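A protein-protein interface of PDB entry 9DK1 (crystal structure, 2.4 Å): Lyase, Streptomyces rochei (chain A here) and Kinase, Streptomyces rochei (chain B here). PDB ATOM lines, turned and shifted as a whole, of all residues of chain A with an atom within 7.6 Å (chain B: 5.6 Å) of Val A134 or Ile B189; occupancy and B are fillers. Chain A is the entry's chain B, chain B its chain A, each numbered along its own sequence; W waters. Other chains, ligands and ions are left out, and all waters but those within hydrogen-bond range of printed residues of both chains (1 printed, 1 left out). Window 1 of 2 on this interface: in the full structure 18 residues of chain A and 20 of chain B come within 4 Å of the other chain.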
ATOM      1  N   GLY A 113      -8.697 -14.786 -19.938  1.00  0.00           N
ATOM      2  CA  GLY A 113      -9.473 -13.666 -20.438  1.00  0.00           C
ATOM      3  C   GLY A 113      -8.622 -12.400 -20.552  1.00  0.00           C
ATOM      4  O   GLY A 113      -7.423 -12.445 -20.304  1.00  0.00           O
ATOM      5  N   VAL A 129     -12.640  -9.385 -15.407  1.00  0.00           N
ATOM      6  CA  VAL A 129     -11.969  -9.991 -16.582  1.00  0.00           C
ATOM      7  C   VAL A 129     -13.026 -10.366 -17.611  1.00  0.00           C
ATOM      8  O   VAL A 129     -14.038 -10.950 -17.231  1.00  0.00           O
ATOM      9  CB  VAL A 129     -11.134 -11.211 -16.148  1.00  0.00           C
ATOM     10  CG1 VAL A 129     -10.658 -12.028 -17.336  1.00  0.00           C
ATOM     11  CG2 VAL A 129      -9.974 -10.820 -15.252  1.00  0.00           C
ATOM     12  N   ARG A 130     -12.777 -10.012 -18.866  1.00  0.00           N
ATOM     13  CA  ARG A 130     -13.696 -10.424 -19.943  1.00  0.00           C
ATOM     14  C   ARG A 130     -13.358 -11.849 -20.345  1.00  0.00           C
ATOM     15  O   ARG A 130     -12.420 -12.035 -21.110  1.00  0.00           O
ATOM     16  CB  ARG A 130     -13.647  -9.488 -21.147  1.00  0.00           C
ATOM     17  CG  ARG A 130     -14.647  -9.859 -22.229  1.00  0.00           C
ATOM     18  CD  ARG A 130     -14.433  -9.148 -23.546  1.00  0.00           C
ATOM     19  NE  ARG A 130     -15.476  -9.559 -24.467  1.00  0.00           N
ATOM     20  CZ  ARG A 130     -16.725  -9.123 -24.421  1.00  0.00           C
ATOM     21  NH1 ARG A 130     -17.081  -8.238 -23.508  1.00  0.00           N
ATOM     22  NH2 ARG A 130     -17.610  -9.565 -25.292  1.00  0.00           N
ATOM     23  N   LEU A 131     -14.088 -12.806 -19.801  1.00  0.00           N
ATOM     24  CA  LEU A 131     -13.947 -14.185 -20.200  1.00  0.00           C
ATOM     25  C   LEU A 131     -14.633 -14.291 -21.548  1.00  0.00           C
ATOM     26  O   LEU A 131     -15.334 -13.361 -21.965  1.00  0.00           O
ATOM     27  CB  LEU A 131     -14.571 -15.102 -19.141  1.00  0.00           C
ATOM     28  CG  LEU A 131     -14.045 -14.948 -17.719  1.00  0.00           C
ATOM     29  CD1 LEU A 131     -14.740 -15.913 -16.765  1.00  0.00           C
ATOM     30  CD2 LEU A 131     -12.555 -15.180 -17.686  1.00  0.00           C
ATOM     31  N   PRO A 132     -14.420 -15.386 -22.299  1.00  0.00           N
ATOM     32  CA  PRO A 132     -15.118 -15.555 -23.574  1.00  0.00           C
ATOM     33  C   PRO A 132     -16.645 -15.463 -23.458  1.00  0.00           C
ATOM     34  O   PRO A 132     -17.284 -14.932 -24.362  1.00  0.00           O
ATOM     35  CB  PRO A 132     -14.660 -16.947 -24.047  1.00  0.00           C
ATOM     36  CG  PRO A 132     -13.343 -17.163 -23.350  1.00  0.00           C
ATOM     37  CD  PRO A 132     -13.470 -16.466 -22.008  1.00  0.00           C
ATOM     38  N   GLU A 133     -17.214 -15.988 -22.379  1.00  0.00           N
ATOM     39  CA  GLU A 133     -18.691 -16.084 -22.272  1.00  0.00           C
ATOM     40  C   GLU A 133     -19.300 -14.981 -21.410  1.00  0.00           C
ATOM     41  O   GLU A 133     -20.519 -14.858 -21.428  1.00  0.00           O
ATOM     42  CB  GLU A 133     -19.030 -17.444 -21.670  1.00  0.00           C
ATOM     43  CG  GLU A 133     -18.306 -18.598 -22.337  1.00  0.00           C
ATOM     44  CD  GLU A 133     -16.867 -18.803 -21.897  1.00  0.00           C
ATOM     45  OE1 GLU A 133     -16.414 -18.076 -20.995  1.00  0.00           O
ATOM     46  OE2 GLU A 133     -16.200 -19.687 -22.463  1.00  0.00           O
ATOM     47  N   VAL A 134     -18.484 -14.240 -20.675  1.00  0.00           N
ATOM     48  CA  VAL A 134     -19.033 -13.220 -19.746  1.00  0.00           C
ATOM     49  C   VAL A 134     -17.920 -12.421 -19.099  1.00  0.00           C
ATOM     50  O   VAL A 134     -16.828 -12.950 -18.967  1.00  0.00           O
ATOM     51  CB  VAL A 134     -19.883 -13.889 -18.644  1.00  0.00           C
ATOM     52  CG1 VAL A 134     -19.029 -14.517 -17.558  1.00  0.00           C
ATOM     53  CG2 VAL A 134     -20.908 -12.942 -18.049  1.00  0.00           C
ATOM     54  N   THR A 135     -18.173 -11.154 -18.823  1.00  0.00           N
ATOM     55  CA  THR A 135     -17.270 -10.405 -17.979  1.00  0.00           C
ATOM     56  C   THR A 135     -17.584 -10.774 -16.530  1.00  0.00           C
ATOM     57  O   THR A 135     -18.728 -10.724 -16.107  1.00  0.00           O
ATOM     58  CB  THR A 135     -17.407  -8.910 -18.251  1.00  0.00           C
ATOM     59  OG1 THR A 135     -17.084  -8.681 -19.620  1.00  0.00           O
ATOM     60  CG2 THR A 135     -16.500  -8.073 -17.372  1.00  0.00           C
ATOM     61  N   ALA A 136     -16.555 -11.191 -15.790  1.00  0.00           N
ATOM     62  CA  ALA A 136     -16.698 -11.708 -14.442  1.00  0.00           C
ATOM     63  C   ALA A 136     -15.755 -10.968 -13.489  1.00  0.00           C
ATOM     64  O   ALA A 136     -14.710 -10.433 -13.861  1.00  0.00           O
ATOM     65  CB  ALA A 136     -16.392 -13.182 -14.440  1.00  0.00           C
ATOM     66  N   ARG A 137     -16.161 -10.946 -12.230  1.00  0.00           N
ATOM     67  CA  ARG A 137     -15.396 -10.353 -11.157  1.00  0.00           C
ATOM     68  C   ARG A 137     -14.801 -11.535 -10.410  1.00  0.00           C
ATOM     69  O   ARG A 137     -15.551 -12.327  -9.856  1.00  0.00           O
ATOM     70  CB  ARG A 137     -16.348  -9.515 -10.299  1.00  0.00           C
ATOM     71  CG  ARG A 137     -15.707  -8.434  -9.446  1.00  0.00           C
ATOM     72  CD  ARG A 137     -16.784  -7.684  -8.659  1.00  0.00           C
ATOM     73  NE  ARG A 137     -17.331  -8.377  -7.490  1.00  0.00           N
ATOM     74  CZ  ARG A 137     -18.620  -8.488  -7.205  1.00  0.00           C
ATOM     75  NH1 ARG A 137     -19.000  -8.950  -6.021  1.00  0.00           N
ATOM     76  NH2 ARG A 137     -19.519  -8.103  -8.102  1.00  0.00           N
ATOM     77  N   ARG A 164     -18.858 -27.277 -12.815  1.00  0.00           N
ATOM     78  CA  ARG A 164     -19.917 -26.328 -13.096  1.00  0.00           C
ATOM     79  C   ARG A 164     -21.259 -27.065 -12.996  1.00  0.00           C
ATOM     80  O   ARG A 164     -21.786 -27.585 -13.976  1.00  0.00           O
ATOM     81  CB  ARG A 164     -19.660 -25.696 -14.464  1.00  0.00           C
ATOM     82  CG  ARG A 164     -18.299 -25.032 -14.617  1.00  0.00           C
ATOM     83  CD  ARG A 164     -18.111 -23.809 -13.737  1.00  0.00           C
ATOM     84  NE  ARG A 164     -16.739 -23.315 -13.781  1.00  0.00           N
ATOM     85  CZ  ARG A 164     -16.193 -22.680 -14.813  1.00  0.00           C
ATOM     86  NH1 ARG A 164     -16.956 -22.105 -15.736  1.00  0.00           N
ATOM     87  NH2 ARG A 164     -14.877 -22.613 -14.907  1.00  0.00           N
ATOM     88  N   ALA A 166     -24.414 -26.034 -12.334  1.00  0.00           N
ATOM     89  CA  ALA A 166     -25.588 -25.299 -12.800  1.00  0.00           C
ATOM     90  C   ALA A 166     -25.507 -25.006 -14.295  1.00  0.00           C
ATOM     91  O   ALA A 166     -26.512 -24.673 -14.896  1.00  0.00           O
ATOM     92  CB  ALA A 166     -25.723 -23.994 -12.029  1.00  0.00           C
ATOM     93  N   LEU A 167     -24.321 -25.137 -14.898  1.00  0.00           N
ATOM     94  CA  LEU A 167     -24.092 -24.651 -16.248  1.00  0.00           C
ATOM     95  C   LEU A 167     -25.088 -25.267 -17.235  1.00  0.00           C
ATOM     96  O   LEU A 167     -25.701 -24.574 -18.050  1.00  0.00           O
ATOM     97  CB  LEU A 167     -22.645 -24.949 -16.636  1.00  0.00           C
ATOM     98  CG  LEU A 167     -22.236 -24.410 -18.013  1.00  0.00           C
ATOM     99  CD1 LEU A 167     -22.441 -22.910 -18.100  1.00  0.00           C
ATOM    100  CD2 LEU A 167     -20.782 -24.759 -18.349  1.00  0.00           C
ATOM    101  N   LEU B 176     -20.286  -9.898 -13.609  1.00  0.00           N
ATOM    102  CA  LEU B 176     -20.871 -10.828 -12.655  1.00  0.00           C
ATOM    103  C   LEU B 176     -19.848 -11.252 -11.612  1.00  0.00           C
ATOM    104  O   LEU B 176     -18.730 -11.605 -11.962  1.00  0.00           O
ATOM    105  CB  LEU B 176     -21.340 -12.101 -13.363  1.00  0.00           C
ATOM    106  CG  LEU B 176     -22.830 -12.155 -13.686  1.00  0.00           C
ATOM    107  CD1 LEU B 176     -23.211 -10.981 -14.564  1.00  0.00           C
ATOM    108  CD2 LEU B 176     -23.166 -13.483 -14.350  1.00  0.00           C
ATOM    109  N   VAL B 181     -21.621 -16.574 -11.402  1.00  0.00           N
ATOM    110  CA  VAL B 181     -21.421 -17.318 -12.629  1.00  0.00           C
ATOM    111  C   VAL B 181     -21.519 -18.824 -12.355  1.00  0.00           C
ATOM    112  O   VAL B 181     -22.037 -19.574 -13.179  1.00  0.00           O
ATOM    113  CB  VAL B 181     -20.072 -16.974 -13.279  1.00  0.00           C
ATOM    114  CG1 VAL B 181     -19.799 -17.878 -14.466  1.00  0.00           C
ATOM    115  CG2 VAL B 181     -19.995 -15.521 -13.692  1.00  0.00           C
ATOM    116  N   ARG B 184     -25.245 -20.289 -12.309  1.00  0.00           N
ATOM    117  CA  ARG B 184     -26.140 -19.961 -13.401  1.00  0.00           C
ATOM    118  C   ARG B 184     -25.939 -20.919 -14.571  1.00  0.00           C
ATOM    119  O   ARG B 184     -24.869 -21.504 -14.738  1.00  0.00           O
ATOM    120  CB  ARG B 184     -25.823 -18.585 -13.978  1.00  0.00           C
ATOM    121  CG  ARG B 184     -25.958 -17.445 -12.994  1.00  0.00           C
ATOM    122  CD  ARG B 184     -27.397 -17.179 -12.683  1.00  0.00           C
ATOM    123  NE  ARG B 184     -27.498 -15.967 -11.892  1.00  0.00           N
ATOM    124  CZ  ARG B 184     -27.253 -15.907 -10.598  1.00  0.00           C
ATOM    125  NH1 ARG B 184     -26.389 -16.739 -10.042  1.00  0.00           N
ATOM    126  NH2 ARG B 184     -27.878 -15.000  -9.877  1.00  0.00           N
ATOM    127  N   SER B 185     -26.953 -20.953 -15.424  1.00  0.00           N
ATOM    128  CA  SER B 185     -26.921 -21.771 -16.650  1.00  0.00           C
ATOM    129  C   SER B 185     -26.126 -21.074 -17.747  1.00  0.00           C
ATOM    130  O   SER B 185     -25.847 -19.887 -17.605  1.00  0.00           O
ATOM    131  CB  SER B 185     -28.322 -21.994 -17.105  1.00  0.00           C
ATOM    132  OG  SER B 185     -28.860 -20.831 -17.699  1.00  0.00           O
ATOM    133  N   MET B 186     -25.825 -21.798 -18.814  1.00  0.00           N
ATOM    134  CA  MET B 186     -25.104 -21.246 -19.978  1.00  0.00           C
ATOM    135  C   MET B 186     -25.978 -20.199 -20.660  1.00  0.00           C
ATOM    136  O   MET B 186     -25.440 -19.226 -21.164  1.00  0.00           O
ATOM    137  CB  MET B 186     -24.845 -22.397 -20.950  1.00  0.00           C
ATOM    138  CG  MET B 186     -23.750 -22.191 -21.952  1.00  0.00           C
ATOM    139  SD  MET B 186     -23.547 -23.723 -22.892  1.00  0.00           S
ATOM    140  CE  MET B 186     -23.189 -23.056 -24.516  1.00  0.00           C
ATOM    141  N   ALA B 187     -27.280 -20.427 -20.672  1.00  0.00           N
ATOM    142  CA  ALA B 187     -28.171 -19.482 -21.307  1.00  0.00           C
ATOM    143  C   ALA B 187     -28.226 -18.193 -20.487  1.00  0.00           C
ATOM    144  O   ALA B 187     -28.226 -17.106 -21.033  1.00  0.00           O
ATOM    145  CB  ALA B 187     -29.540 -20.117 -21.419  1.00  0.00           C
ATOM    146  N   GLN B 188     -28.291 -18.324 -19.163  1.00  0.00           N
ATOM    147  CA  GLN B 188     -28.266 -17.165 -18.298  1.00  0.00           C
ATOM    148  C   GLN B 188     -26.982 -16.397 -18.472  1.00  0.00           C
ATOM    149  O   GLN B 188     -27.021 -15.176 -18.568  1.00  0.00           O
ATOM    150  CB  GLN B 188     -28.374 -17.550 -16.833  1.00  0.00           C
ATOM    151  CG  GLN B 188     -29.775 -18.015 -16.465  1.00  0.00           C
ATOM    152  CD  GLN B 188     -29.820 -18.334 -14.986  1.00  0.00           C
ATOM    153  OE1 GLN B 188     -29.067 -19.156 -14.472  1.00  0.00           O
ATOM    154  NE2 GLN B 188     -30.688 -17.658 -14.273  1.00  0.00           N
ATOM    155  N   ILE B 189     -25.862 -17.124 -18.494  1.00  0.00           N
ATOM    156  CA  ILE B 189     -24.561 -16.500 -18.675  1.00  0.00           C
ATOM    157  C   ILE B 189     -24.479 -15.755 -20.007  1.00  0.00           C
ATOM    158  O   ILE B 189     -23.972 -14.632 -20.042  1.00  0.00           O
ATOM    159  CB  ILE B 189     -23.466 -17.556 -18.495  1.00  0.00           C
ATOM    160  CG1 ILE B 189     -23.454 -18.076 -17.051  1.00  0.00           C
ATOM    161  CG2 ILE B 189     -22.116 -16.991 -18.888  1.00  0.00           C
ATOM    162  CD1 ILE B 189     -22.555 -19.272 -16.866  1.00  0.00           C
ATOM    163  N   ALA B 190     -25.069 -16.344 -21.067  1.00  0.00           N
ATOM    164  CA  ALA B 190     -25.135 -15.756 -22.402  1.00  0.00           C
ATOM    165  C   ALA B 190     -26.032 -14.526 -22.419  1.00  0.00           C
ATOM    166  O   ALA B 190     -25.711 -13.529 -23.036  1.00  0.00           O
ATOM    167  CB  ALA B 190     -25.636 -16.773 -23.397  1.00  0.00           C
ATOM    168  N   ALA B 191     -27.150 -14.599 -21.709  1.00  0.00           N
ATOM    169  CA  ALA B 191     -28.074 -13.481 -21.561  1.00  0.00           C
ATOM    170  C   ALA B 191     -27.410 -12.321 -20.803  1.00  0.00           C
ATOM    171  O   ALA B 191     -27.590 -11.172 -21.166  1.00  0.00           O
ATOM    172  CB  ALA B 191     -29.305 -13.985 -20.844  1.00  0.00           C
ATOM    173  N   TRP B 192     -26.626 -12.616 -19.757  1.00  0.00           N
ATOM    174  CA  TRP B 192     -25.856 -11.595 -19.069  1.00  0.00           C
ATOM    175  C   TRP B 192     -24.829 -10.939 -19.983  1.00  0.00           C
ATOM    176  O   TRP B 192     -24.688  -9.719 -19.976  1.00  0.00           O
ATOM    177  CB  TRP B 192     -25.208 -12.157 -17.805  1.00  0.00           C
ATOM    178  CG  TRP B 192     -26.176 -12.171 -16.662  1.00  0.00           C
ATOM    179  CD1 TRP B 192     -26.749 -13.242 -16.018  1.00  0.00           C
ATOM    180  CD2 TRP B 192     -26.712 -10.988 -16.039  1.00  0.00           C
ATOM    181  NE1 TRP B 192     -27.605 -12.796 -15.033  1.00  0.00           N
ATOM    182  CE2 TRP B 192     -27.590 -11.419 -15.021  1.00  0.00           C
ATOM    183  CE3 TRP B 192     -26.512  -9.614 -16.246  1.00  0.00           C
ATOM    184  CZ2 TRP B 192     -28.291 -10.500 -14.240  1.00  0.00           C
ATOM    185  CZ3 TRP B 192     -27.193  -8.716 -15.460  1.00  0.00           C
ATOM    186  CH2 TRP B 192     -28.085  -9.158 -14.487  1.00  0.00           C
ATOM    187  N   GLN B 193     -24.084 -11.723 -20.748  1.00  0.00           N
ATOM    188  CA  GLN B 193     -23.011 -11.158 -21.603  1.00  0.00           C
ATOM    189  C   GLN B 193     -23.605 -10.249 -22.674  1.00  0.00           C
ATOM    190  O   GLN B 193     -23.004  -9.229 -22.985  1.00  0.00           O
ATOM    191  CB  GLN B 193     -22.213 -12.270 -22.268  1.00  0.00           C
ATOM    192  CG  GLN B 193     -21.167 -11.762 -23.245  1.00  0.00           C
ATOM    193  CD  GLN B 193     -20.632 -12.864 -24.121  1.00  0.00           C
ATOM    194  OE1 GLN B 193     -21.382 -13.583 -24.773  1.00  0.00           O
ATOM    195  NE2 GLN B 193     -19.319 -13.010 -24.133  1.00  0.00           N
ATOM    196  N   LEU B 194     -24.763 -10.619 -23.190  1.00  0.00           N
ATOM    197  CA  LEU B 194     -25.391  -9.820 -24.253  1.00  0.00           C
ATOM    198  C   LEU B 194     -25.754  -8.443 -23.698  1.00  0.00           C
ATOM    199  O   LEU B 194     -25.632  -7.467 -24.435  1.00  0.00           O
ATOM    200  CB  LEU B 194     -26.619 -10.579 -24.751  1.00  0.00           C
ATOM    201  CG  LEU B 194     -26.337 -11.692 -25.755  1.00  0.00           C
ATOM    202  CD1 LEU B 194     -27.574 -12.540 -25.982  1.00  0.00           C
ATOM    203  CD2 LEU B 194     -25.838 -11.115 -27.069  1.00  0.00           C
ATOM    204  N   GLN B 196     -24.280  -7.024 -20.892  1.00  0.00           N
ATOM    205  CA  GLN B 196     -23.018  -6.380 -20.551  1.00  0.00           C
ATOM    206  C   GLN B 196     -22.411  -5.699 -21.783  1.00  0.00           C
ATOM    207  O   GLN B 196     -21.926  -4.579 -21.670  1.00  0.00           O
ATOM    208  CB  GLN B 196     -21.998  -7.357 -19.949  1.00  0.00           C
ATOM    209  CG  GLN B 196     -22.397  -7.944 -18.594  1.00  0.00           C
ATOM    210  CD  GLN B 196     -21.482  -9.069 -18.156  1.00  0.00           C
ATOM    211  OE1 GLN B 196     -20.935  -9.798 -18.976  1.00  0.00           O
ATOM    212  NE2 GLN B 196     -21.204  -9.144 -16.862  1.00  0.00           N
HETATM  213  O   HOH W   1     -19.206  -9.318 -21.321  1.00  0.00           O
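The backbone carbonyl oxygen (O) of Thr A135 is in hydrogen-bond range of the backbone NH (N) of Leu B176, 3.1 Å away.
The backbone carbonyl oxygen (O) of Leu B176 is in hydrogen-bond range of the backbone NH (N) of Arg A137, at 2.7 Å.
N of Met B186 lies within hydrogen-bond range of O of Leu A167, at 2.9 Å.
The side-chain amide nitrogen (NE2) of Gln B193 is in hydrogen-bond range of the backbone carbonyl oxygen (O) of Pro A132 (2.8 Å).
The backbone carbonyl oxygen (O) of Glu A133 sits close to the side-chain amide nitrogen (NE2) of Gln B193 (3.5 Å).
The side-chain amide nitrogen (NE2) of Gln B196 sits at hydrogen-bond distance from the backbone carbonyl oxygen (O) of Thr A135, 3.0 Å away.
Printed residues of chain B that touch a printed residue of chain A: Leu B176, Arg B184, Ser B185, Met B186, Ile B189, Gln B193 and Gln B196.
Along chain A the printed residues that touch a printed residue of chain B span positions 132 to 167.
Among the printed residues, 16 pairs touch across the chains.
Among the printed residues, no Asp or Glu carboxylate lies within 4 Å of a Lys or Arg side-chain nitrogen of the other chain.
N of Leu B176 lies close to NE2 of Gln B196 (3.5 Å).
OG of Ser B185 sits close to N of Ala B187 (3.4 Å).
The side-chain amide oxygen of Gln B188 lies within hydrogen-bond range of the backbone NH of Ser B185, at 2.9 Å.
N of Val A129 is in hydrogen-bond range of O of Ala A136 (2.8 Å).
O of Glu A133 touches CG2 of Ile B189 (3.7 Å).
Val A134 touches Ile B189.
Val A134 touches Gln B193 (N to NE2, 3.8 Å).
Gln B196 touches Val A134 (OE1 to CG2, 3.3 Å).
CA of Ala A136 touches O of Leu B176, at 3.2 Å.
O of Arg B184 touches O of Ala A166, at 3.6 Å.
Ala A166 touches Ser B185.
Leu A167 touches Arg B184 (CA to O, 3.6 Å).
Ser B185 touches Leu A167 (CA to O, 3.4 Å).
CD1 of Ile B189 touches CD1 of Leu A167 (3.8 Å).
Water W1 lies within hydrogen-bond range of the side-chain hydroxyl of Thr A135, the side-chain amide oxygen of Gln B196 and the guanidinium group of Arg A130.
Of chain B, only Ile B189 (3.8 Å), Gln B193 (3.8 Å) and Gln B196 (3.3 Å) come within 4 Å of Val A134.
Ile B189 touches just these residues of chain A: Glu A133, Val A134 and Leu A167.
Of the printed residues of chain B, Ala A136 touches Leu B176.
Printed residues of chain B within 4 Å of Ala A166: Arg B184 and Ser B185.
Arg A130 touches none of the printed residues of chain B.
The nearest residue of chain B that does not touch Val A134 is Val B181 (4.1 Å).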
